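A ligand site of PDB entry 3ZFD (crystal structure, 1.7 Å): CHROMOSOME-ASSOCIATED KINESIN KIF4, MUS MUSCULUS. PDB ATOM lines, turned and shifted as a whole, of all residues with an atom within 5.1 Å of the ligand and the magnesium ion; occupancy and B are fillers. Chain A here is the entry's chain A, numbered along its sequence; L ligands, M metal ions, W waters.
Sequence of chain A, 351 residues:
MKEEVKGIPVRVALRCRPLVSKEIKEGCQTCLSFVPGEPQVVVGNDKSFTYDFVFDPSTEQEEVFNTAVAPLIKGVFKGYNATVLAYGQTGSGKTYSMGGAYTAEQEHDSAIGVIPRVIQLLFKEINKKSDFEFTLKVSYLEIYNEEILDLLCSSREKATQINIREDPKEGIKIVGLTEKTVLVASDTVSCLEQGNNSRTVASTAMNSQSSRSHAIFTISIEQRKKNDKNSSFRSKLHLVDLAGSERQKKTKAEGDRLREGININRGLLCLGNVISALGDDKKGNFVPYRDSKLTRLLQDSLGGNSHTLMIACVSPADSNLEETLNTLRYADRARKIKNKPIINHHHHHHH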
ATOM      1  N   ARG A  15      11.636 -20.546  21.128  1.00  0.00           N
ATOM      2  CA  ARG A  15      12.170 -19.465  20.323  1.00  0.00           C
ATOM      3  C   ARG A  15      12.984 -19.989  19.191  1.00  0.00           C
ATOM      4  O   ARG A  15      14.010 -20.632  19.392  1.00  0.00           O
ATOM      5  CB  ARG A  15      12.995 -18.477  21.094  1.00  0.00           C
ATOM      6  CG  ARG A  15      13.420 -17.359  20.120  1.00  0.00           C
ATOM      7  CD  ARG A  15      14.381 -16.426  20.713  1.00  0.00           C
ATOM      8  NE  ARG A  15      14.384 -15.141  20.028  1.00  0.00           N
ATOM      9  CZ  ARG A  15      15.085 -14.093  20.421  1.00  0.00           C
ATOM     10  NH1 ARG A  15      15.916 -14.189  21.447  1.00  0.00           N
ATOM     11  NH2 ARG A  15      14.987 -12.947  19.764  1.00  0.00           N
ATOM     12  N   ARG A  17      15.288 -19.001  16.091  1.00  0.00           N
ATOM     13  CA  ARG A  17      16.102 -17.914  15.563  1.00  0.00           C
ATOM     14  C   ARG A  17      16.053 -17.993  14.056  1.00  0.00           C
ATOM     15  O   ARG A  17      15.613 -18.980  13.489  1.00  0.00           O
ATOM     16  CB  ARG A  17      17.535 -18.070  16.043  1.00  0.00           C
ATOM     17  CG  ARG A  17      18.227 -19.367  15.631  1.00  0.00           C
ATOM     18  CD  ARG A  17      19.712 -19.110  15.573  1.00  0.00           C
ATOM     19  NE  ARG A  17      20.515 -20.313  15.417  1.00  0.00           N
ATOM     20  CZ  ARG A  17      20.611 -21.051  14.323  1.00  0.00           C
ATOM     21  NH1 ARG A  17      19.976 -20.715  13.207  1.00  0.00           N
ATOM     22  NH2 ARG A  17      21.375 -22.124  14.319  1.00  0.00           N
ATOM     23  N   PRO A  18      16.503 -16.935  13.378  1.00  0.00           N
ATOM     24  CA  PRO A  18      16.666 -17.031  11.934  1.00  0.00           C
ATOM     25  C   PRO A  18      17.787 -17.981  11.539  1.00  0.00           C
ATOM     26  O   PRO A  18      18.660 -18.300  12.359  1.00  0.00           O
ATOM     27  CB  PRO A  18      17.051 -15.603  11.528  1.00  0.00           C
ATOM     28  CG  PRO A  18      16.925 -14.761  12.728  1.00  0.00           C
ATOM     29  CD  PRO A  18      16.913 -15.632  13.916  1.00  0.00           C
ATOM     30  N   VAL A  20      21.326 -18.903  10.181  1.00  0.00           N
ATOM     31  CA  VAL A  20      22.607 -18.268  10.368  1.00  0.00           C
ATOM     32  C   VAL A  20      23.486 -18.583   9.157  1.00  0.00           C
ATOM     33  O   VAL A  20      23.151 -19.434   8.326  1.00  0.00           O
ATOM     34  CB  VAL A  20      23.310 -18.712  11.661  1.00  0.00           C
ATOM     35  CG1 VAL A  20      22.514 -18.251  12.886  1.00  0.00           C
ATOM     36  CG2 VAL A  20      23.522 -20.222  11.701  1.00  0.00           C
ATOM     37  N   GLY A  88      18.714 -25.901  24.560  1.00  0.00           N
ATOM     38  CA  GLY A  88      18.726 -26.200  23.121  1.00  0.00           C
ATOM     39  C   GLY A  88      20.101 -26.511  22.593  1.00  0.00           C
ATOM     40  O   GLY A  88      21.108 -26.351  23.283  1.00  0.00           O
ATOM     41  N   GLN A  89      20.142 -26.934  21.329  1.00  0.00           N
ATOM     42  CA  GLN A  89      21.368 -27.360  20.666  1.00  0.00           C
ATOM     43  C   GLN A  89      22.430 -26.253  20.640  1.00  0.00           C
ATOM     44  O   GLN A  89      22.088 -25.081  20.681  1.00  0.00           O
ATOM     45  CB  GLN A  89      20.957 -27.683  19.227  1.00  0.00           C
ATOM     46  CG  GLN A  89      22.016 -28.154  18.273  1.00  0.00           C
ATOM     47  CD  GLN A  89      21.612 -28.021  16.804  1.00  0.00           C
ATOM     48  OE1 GLN A  89      20.624 -27.355  16.399  1.00  0.00           O
ATOM     49  NE2 GLN A  89      22.356 -28.706  15.987  1.00  0.00           N
ATOM     50  N   THR A  90      23.703 -26.627  20.546  1.00  0.00           N
ATOM     51  CA  THR A  90      24.720 -25.611  20.255  1.00  0.00           C
ATOM     52  C   THR A  90      24.338 -24.746  19.049  1.00  0.00           C
ATOM     53  O   THR A  90      23.869 -25.233  18.027  1.00  0.00           O
ATOM     54  CB  THR A  90      26.130 -26.245  20.054  1.00  0.00           C
ATOM     55  OG1 THR A  90      27.114 -25.212  19.866  1.00  0.00           O
ATOM     56  CG2 THR A  90      26.153 -27.178  18.852  1.00  0.00           C
ATOM     57  N   GLY A  91      24.525 -23.434  19.199  1.00  0.00           N
ATOM     58  CA  GLY A  91      24.265 -22.496  18.140  1.00  0.00           C
ATOM     59  C   GLY A  91      22.821 -22.075  17.997  1.00  0.00           C
ATOM     60  O   GLY A  91      22.528 -21.252  17.138  1.00  0.00           O
ATOM     61  N   SER A  92      21.931 -22.638  18.820  1.00  0.00           N
ATOM     62  CA  SER A  92      20.484 -22.334  18.742  1.00  0.00           C
ATOM     63  C   SER A  92      20.050 -20.944  19.201  1.00  0.00           C
ATOM     64  O   SER A  92      19.001 -20.468  18.728  1.00  0.00           O
ATOM     65  CB  SER A  92      19.625 -23.383  19.442  1.00  0.00           C
ATOM     66  OG  SER A  92      19.974 -23.511  20.793  1.00  0.00           O
ATOM     67  N   GLY A  93      20.828 -20.308  20.087  1.00  0.00           N
ATOM     68  CA  GLY A  93      20.582 -18.932  20.539  1.00  0.00           C
ATOM     69  C   GLY A  93      20.312 -18.759  22.020  1.00  0.00           C
ATOM     70  O   GLY A  93      19.707 -17.769  22.412  1.00  0.00           O
ATOM     71  N   LYS A  94      20.766 -19.689  22.852  1.00  0.00           N
ATOM     72  CA  LYS A  94      20.593 -19.618  24.312  1.00  0.00           C
ATOM     73  C   LYS A  94      21.308 -18.392  24.915  1.00  0.00           C
ATOM     74  O   LYS A  94      20.713 -17.605  25.633  1.00  0.00           O
ATOM     75  CB  LYS A  94      21.136 -20.868  24.983  1.00  0.00           C
ATOM     76  CG  LYS A  94      20.476 -22.205  24.560  1.00  0.00           C
ATOM     77  CD  LYS A  94      21.087 -23.398  25.263  1.00  0.00           C
ATOM     78  CE  LYS A  94      22.530 -23.658  24.831  1.00  0.00           C
ATOM     79  NZ  LYS A  94      22.685 -23.927  23.391  1.00  0.00           N
ATOM     80  N   THR A  95      22.589 -18.245  24.604  1.00  0.00           N
ATOM     81  CA  THR A  95      23.386 -17.132  25.159  1.00  0.00           C
ATOM     82  C   THR A  95      22.854 -15.811  24.617  1.00  0.00           C
ATOM     83  O   THR A  95      22.686 -14.838  25.365  1.00  0.00           O
ATOM     84  CB  THR A  95      24.864 -17.340  24.815  1.00  0.00           C
ATOM     85  OG1 THR A  95      25.344 -18.508  25.486  1.00  0.00           O
ATOM     86  CG2 THR A  95      25.737 -16.170  25.278  1.00  0.00           C
ATOM     87  N   TYR A  96      22.563 -15.783  23.320  1.00  0.00           N
ATOM     88  CA  TYR A  96      21.958 -14.631  22.686  1.00  0.00           C
ATOM     89  C   TYR A  96      20.671 -14.249  23.385  1.00  0.00           C
ATOM     90  O   TYR A  96      20.449 -13.067  23.718  1.00  0.00           O
ATOM     91  CB  TYR A  96      21.698 -14.904  21.210  1.00  0.00           C
ATOM     92  CG  TYR A  96      21.027 -13.750  20.521  1.00  0.00           C
ATOM     93  CD1 TYR A  96      21.781 -12.704  20.038  1.00  0.00           C
ATOM     94  CD2 TYR A  96      19.652 -13.682  20.369  1.00  0.00           C
ATOM     95  CE1 TYR A  96      21.194 -11.637  19.408  1.00  0.00           C
ATOM     96  CE2 TYR A  96      19.061 -12.626  19.732  1.00  0.00           C
ATOM     97  CZ  TYR A  96      19.825 -11.606  19.253  1.00  0.00           C
ATOM     98  OH  TYR A  96      19.263 -10.507  18.614  1.00  0.00           O
ATOM     99  N   SER A  97      19.817 -15.234  23.631  1.00  0.00           N
ATOM    100  CA  SER A  97      18.509 -14.949  24.259  1.00  0.00           C
ATOM    101  C   SER A  97      18.671 -14.468  25.695  1.00  0.00           C
ATOM    102  O   SER A  97      17.929 -13.604  26.157  1.00  0.00           O
ATOM    103  CB  SER A  97      17.616 -16.193  24.233  1.00  0.00           C
ATOM    104  OG  SER A  97      17.231 -16.488  22.908  1.00  0.00           O
ATOM    105  N   ARG A 199      33.373 -16.385  31.825  1.00  0.00           N
ATOM    106  CA  ARG A 199      32.692 -17.586  31.337  1.00  0.00           C
ATOM    107  C   ARG A 199      33.569 -18.305  30.329  1.00  0.00           C
ATOM    108  O   ARG A 199      34.155 -17.661  29.461  1.00  0.00           O
ATOM    109  CB  ARG A 199      31.368 -17.212  30.658  1.00  0.00           C
ATOM    110  CG  ARG A 199      30.613 -18.343  29.918  1.00  0.00           C
ATOM    111  CD  ARG A 199      29.701 -18.993  30.893  1.00  0.00           C
ATOM    112  NE  ARG A 199      28.772 -20.008  30.333  1.00  0.00           N
ATOM    113  CZ  ARG A 199      27.630 -19.718  29.712  1.00  0.00           C
ATOM    114  NH1 ARG A 199      27.288 -18.455  29.489  1.00  0.00           N
ATOM    115  NH2 ARG A 199      26.827 -20.703  29.358  1.00  0.00           N
ATOM    116  N   ASN A 207      29.635 -23.096  16.438  1.00  0.00           N
ATOM    117  CA  ASN A 207      29.528 -21.791  17.104  1.00  0.00           C
ATOM    118  C   ASN A 207      30.930 -21.265  17.463  1.00  0.00           C
ATOM    119  O   ASN A 207      31.620 -21.841  18.282  1.00  0.00           O
ATOM    120  CB  ASN A 207      28.614 -21.897  18.351  1.00  0.00           C
ATOM    121  CG  ASN A 207      28.280 -20.535  18.958  1.00  0.00           C
ATOM    122  OD1 ASN A 207      28.851 -19.492  18.608  1.00  0.00           O
ATOM    123  ND2 ASN A 207      27.366 -20.543  19.920  1.00  0.00           N
ATOM    124  N   GLN A 209      31.646 -18.844  19.244  1.00  0.00           N
ATOM    125  CA  GLN A 209      31.607 -18.401  20.637  1.00  0.00           C
ATOM    126  C   GLN A 209      30.750 -19.352  21.471  1.00  0.00           C
ATOM    127  O   GLN A 209      29.843 -18.920  22.201  1.00  0.00           O
ATOM    128  CB  GLN A 209      31.052 -16.990  20.704  1.00  0.00           C
ATOM    129  CG  GLN A 209      31.843 -15.966  19.873  1.00  0.00           C
ATOM    130  CD  GLN A 209      33.118 -15.449  20.525  1.00  0.00           C
ATOM    131  OE1 GLN A 209      33.897 -14.697  19.882  1.00  0.00           O
ATOM    132  NE2 GLN A 209      33.331 -15.791  21.769  1.00  0.00           N
ATOM    133  N   SER A 210      31.029 -20.641  21.347  1.00  0.00           N
ATOM    134  CA  SER A 210      30.296 -21.675  22.051  1.00  0.00           C
ATOM    135  C   SER A 210      30.523 -21.584  23.547  1.00  0.00           C
ATOM    136  O   SER A 210      31.689 -21.498  24.019  1.00  0.00           O
ATOM    137  CB  SER A 210      30.688 -23.062  21.576  1.00  0.00           C
ATOM    138  OG  SER A 210      29.990 -24.043  22.328  1.00  0.00           O
ATOM    139  N   SER A 211      29.432 -21.644  24.312  1.00  0.00           N
ATOM    140  CA  SER A 211      29.559 -21.686  25.772  1.00  0.00           C
ATOM    141  C   SER A 211      30.018 -23.094  26.196  1.00  0.00           C
ATOM    142  O   SER A 211      29.363 -24.089  25.869  1.00  0.00           O
ATOM    143  CB  SER A 211      28.240 -21.377  26.438  1.00  0.00           C
ATOM    144  OG  SER A 211      27.600 -20.236  25.882  1.00  0.00           O
ATOM    145  N   ASP A 241      21.876 -19.912  31.602  1.00  0.00           N
ATOM    146  CA  ASP A 241      22.291 -20.055  30.212  1.00  0.00           C
ATOM    147  C   ASP A 241      23.006 -21.421  30.149  1.00  0.00           C
ATOM    148  O   ASP A 241      24.190 -21.542  30.486  1.00  0.00           O
ATOM    149  CB  ASP A 241      23.192 -18.897  29.804  1.00  0.00           C
ATOM    150  CG  ASP A 241      23.727 -19.015  28.406  1.00  0.00           C
ATOM    151  OD1 ASP A 241      23.130 -19.792  27.610  1.00  0.00           O
ATOM    152  OD2 ASP A 241      24.774 -18.363  28.082  1.00  0.00           O
ATOM    153  N   LEU A 242      22.268 -22.457  29.788  1.00  0.00           N
ATOM    154  CA  LEU A 242      22.854 -23.791  29.681  1.00  0.00           C
ATOM    155  C   LEU A 242      23.824 -23.868  28.505  1.00  0.00           C
ATOM    156  O   LEU A 242      23.690 -23.149  27.537  1.00  0.00           O
ATOM    157  CB  LEU A 242      21.791 -24.862  29.485  1.00  0.00           C
ATOM    158  CG  LEU A 242      20.741 -25.023  30.594  1.00  0.00           C
ATOM    159  CD1 LEU A 242      19.739 -26.063  30.170  1.00  0.00           C
ATOM    160  CD2 LEU A 242      21.423 -25.363  31.910  1.00  0.00           C
ATOM    161  N   ALA A 243      24.785 -24.761  28.619  1.00  0.00           N
ATOM    162  CA  ALA A 243      25.492 -25.258  27.462  1.00  0.00           C
ATOM    163  C   ALA A 243      24.531 -26.153  26.657  1.00  0.00           C
ATOM    164  O   ALA A 243      23.444 -26.519  27.133  1.00  0.00           O
ATOM    165  CB  ALA A 243      26.773 -25.977  27.876  1.00  0.00           C
ATOM    166  N   GLY A 244      24.871 -26.379  25.393  1.00  0.00           N
ATOM    167  CA  GLY A 244      23.974 -27.037  24.442  1.00  0.00           C
ATOM    168  C   GLY A 244      24.514 -28.351  23.926  1.00  0.00           C
ATOM    169  O   GLY A 244      25.735 -28.597  23.904  1.00  0.00           O
HETATM  170  P1  LIG L   1      26.270 -22.867  22.599  1.00  0.00           P
HETATM  171  O1  LIG L   1      26.730 -21.942  23.720  1.00  0.00           O
HETATM  172  O2  LIG L   1      27.402 -23.377  21.748  1.00  0.00           O
HETATM  173  O3  LIG L   1      25.506 -24.049  23.234  1.00  0.00           O
HETATM  174  P2  LIG L   1      24.105 -20.984  21.948  1.00  0.00           P
HETATM  175  O4  LIG L   1      22.714 -21.553  21.883  1.00  0.00           O
HETATM  176  O5  LIG L   1      24.434 -20.173  23.197  1.00  0.00           O
HETATM  177  N1  LIG L   1      25.285 -22.077  21.565  1.00  0.00           N
HETATM  178  P3  LIG L   1      24.415 -18.373  20.752  1.00  0.00           P
HETATM  179  O6  LIG L   1      23.353 -17.697  21.584  1.00  0.00           O
HETATM  180  O7  LIG L   1      25.884 -18.172  20.984  1.00  0.00           O
HETATM  181  O8  LIG L   1      24.166 -19.968  20.705  1.00  0.00           O
HETATM  182  O9  LIG L   1      24.067 -17.976  19.235  1.00  0.00           O
HETATM  183  C1  LIG L   1      24.841 -18.444  18.127  1.00  0.00           C
HETATM  184  C2  LIG L   1      24.875 -17.371  17.029  1.00  0.00           C
HETATM  185  O10 LIG L   1      23.547 -17.197  16.523  1.00  0.00           O
HETATM  186  C3  LIG L   1      25.376 -16.059  17.576  1.00  0.00           C
HETATM  187  O11 LIG L   1      26.288 -15.436  16.627  1.00  0.00           O
HETATM  188  C4  LIG L   1      24.106 -15.273  17.773  1.00  0.00           C
HETATM  189  O12 LIG L   1      24.295 -13.844  17.767  1.00  0.00           O
HETATM  190  C5  LIG L   1      23.201 -15.810  16.665  1.00  0.00           C
HETATM  191  N2  LIG L   1      21.796 -15.769  17.086  1.00  0.00           N
HETATM  192  C6  LIG L   1      21.261 -16.556  18.047  1.00  0.00           C
HETATM  193  N3  LIG L   1      19.960 -16.277  18.205  1.00  0.00           N
HETATM  194  C7  LIG L   1      19.654 -15.277  17.322  1.00  0.00           C
HETATM  195  C8  LIG L   1      18.445 -14.518  16.964  1.00  0.00           C
HETATM  196  N4  LIG L   1      17.273 -14.732  17.554  1.00  0.00           N
HETATM  197  N5  LIG L   1      18.579 -13.577  15.995  1.00  0.00           N
HETATM  198  C9  LIG L   1      19.733 -13.323  15.359  1.00  0.00           C
HETATM  199  N6  LIG L   1      20.882 -13.989  15.633  1.00  0.00           N
HETATM  200  C10 LIG L   1      20.857 -14.980  16.580  1.00  0.00           C
HETATM  201 MG    MG M   1      25.984 -20.306  24.522  1.00  0.00          MG
HETATM  202  O   HOH W   1      25.648 -12.732  19.769  1.00  0.00           O
HETATM  203  O   HOH W   2      16.879 -11.466  15.340  1.00  0.00           O
HETATM  204  O   HOH W   3      28.775 -16.888  17.732  1.00  0.00           O
HETATM  205  O   HOH W   4      15.117 -13.285  16.311  1.00  0.00           O
HETATM  206  O   HOH W   5      27.424 -25.396  24.574  1.00  0.00           O
HETATM  207  O   HOH W   6      17.567 -16.666  19.780  1.00  0.00           O
HETATM  208  O   HOH W   7      27.117 -15.785  21.865  1.00  0.00           O
HETATM  209  O   HOH W   8      25.229 -15.870  13.670  1.00  0.00           O
HETATM  210  O   HOH W   9      22.489 -14.249  13.102  1.00  0.00           O
HETATM  211  O   HOH W  10      24.790 -21.246  26.016  1.00  0.00           O
HETATM  212  O   HOH W  11      27.092 -19.070  23.235  1.00  0.00           O
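The backbone NH (N) of Ser 211 sits close to an oxygen (O1) of the ligand (2.8 Å).
N of Thr 95 is in hydrogen-bond range of O6 of the ligand, 3.2 Å away.
The side-chain hydroxyl (OG1) of Thr 90 lies within hydrogen-bond range of an oxygen (O2) of the ligand, at 2.6 Å.
N of Tyr 96 sits at hydrogen-bond distance from O6 of the ligand (2.7 Å).
The side-chain hydroxyl (OG) of Ser 210 lies within hydrogen-bond range of an oxygen (O2) of the ligand (2.7 Å).
O4 of the ligand lies within hydrogen-bond range of N of Lys 94, 2.9 Å away.
O4 of the ligand lies within salt-bridge range of NZ of Lys 94 (2.8 Å).
The backbone NH (N) of Gly 93 lies within hydrogen-bond range of an oxygen (O4) of the ligand.
The side-chain amide nitrogen (ND2) of Asn 207 is in hydrogen-bond range of an oxygen (O7) of the ligand, at 3.0 Å.
An oxygen (O3) of the ligand is in hydrogen-bond range of the backbone NH (N) of Gly 244 (3.2 Å).
N of Ser 92 is in hydrogen-bond range of O4 of the ligand, at 3.3 Å.
The backbone NH of Gly 91 sits close to a nitrogen (N1) of the ligand.
NH2 of Arg 15 touches N4 of the ligand, 3.6 Å away.
Arg 17 touches the ligand.
CD of Pro 18 touches N5 of the ligand, at 3.4 Å.
CG1 of Val 20 touches O10 of the ligand, 3.9 Å away.
Gln 89 touches the ligand.
Hydrophobic or aromatic side chains within 4 Å of the ligand: Pro 18, Val 20 and Tyr 96.
Water W11 bridges O7 of the ligand (2.7 Å) and O of Gln 209 (2.9 Å).
Water W10 lies within hydrogen-bond range of O of Leu 242 and OD1 of Asp 241.
Water W5 lies within hydrogen-bond range of O of Ser 211 (2.7 Å), O3 of the ligand (2.7 Å) and N of Gly 244 (2.9 Å).
Water W4 lies within hydrogen-bond range of N4 of the ligand and NH2 of Arg 15.
Water W6 lies within hydrogen-bond range of a nitrogen (N3) of the ligand (2.9 Å), the side-chain hydroxyl of Ser 97 (3.2 Å) and the guanidinium group of Arg 15 (3.4 Å).
Water W3 lies within hydrogen-bond range of OD1 of Asn 207 (2.7 Å) and O11 of the ligand (3.1 Å).
The backbone NH (N) of Thr 95 sits at hydrogen-bond distance from the side-chain carboxylate (OD1) of Asp 241 (3.4 Å).
The side-chain amino group of Lys 94 sits at hydrogen-bond distance from the backbone carbonyl oxygen of Gln 89 (3.0 Å).
The side-chain amino group of Lys 94 lies within hydrogen-bond range of the backbone carbonyl oxygen of Gly 88 (2.9 Å).
The backbone carbonyl oxygen (O) of Gly 91 is in hydrogen-bond range of the guanidinium group (NE) of Arg 17, 2.8 Å away.
The side-chain hydroxyl of Ser 97 sits at hydrogen-bond distance from the backbone carbonyl oxygen of Gly 93 (2.8 Å).
The side-chain amide oxygen (OD1) of Asn 207 sits at hydrogen-bond distance from the backbone NH (N) of Gln 209 (2.9 Å).
The side-chain hydroxyl (OG) of Ser 92 lies within hydrogen-bond range of the backbone carbonyl oxygen (O) of Gln 89.
NH1 of Arg 15 sits at hydrogen-bond distance from OG of Ser 97, 3.0 Å away.
The nearest printed residue that does not touch the magnesium ion is Asp 241 (4.2 Å).
The magnesium ion is bound by an oxygen (O1) of the ligand (2.0 Å), an oxygen (O5) of the ligand (2.0 Å), water W11 (2.1 Å), the side-chain hydroxyl of Ser 211 (2.1 Å), water W10 (2.1 Å) and the side-chain hydroxyl of Thr 95 (2.1 Å).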
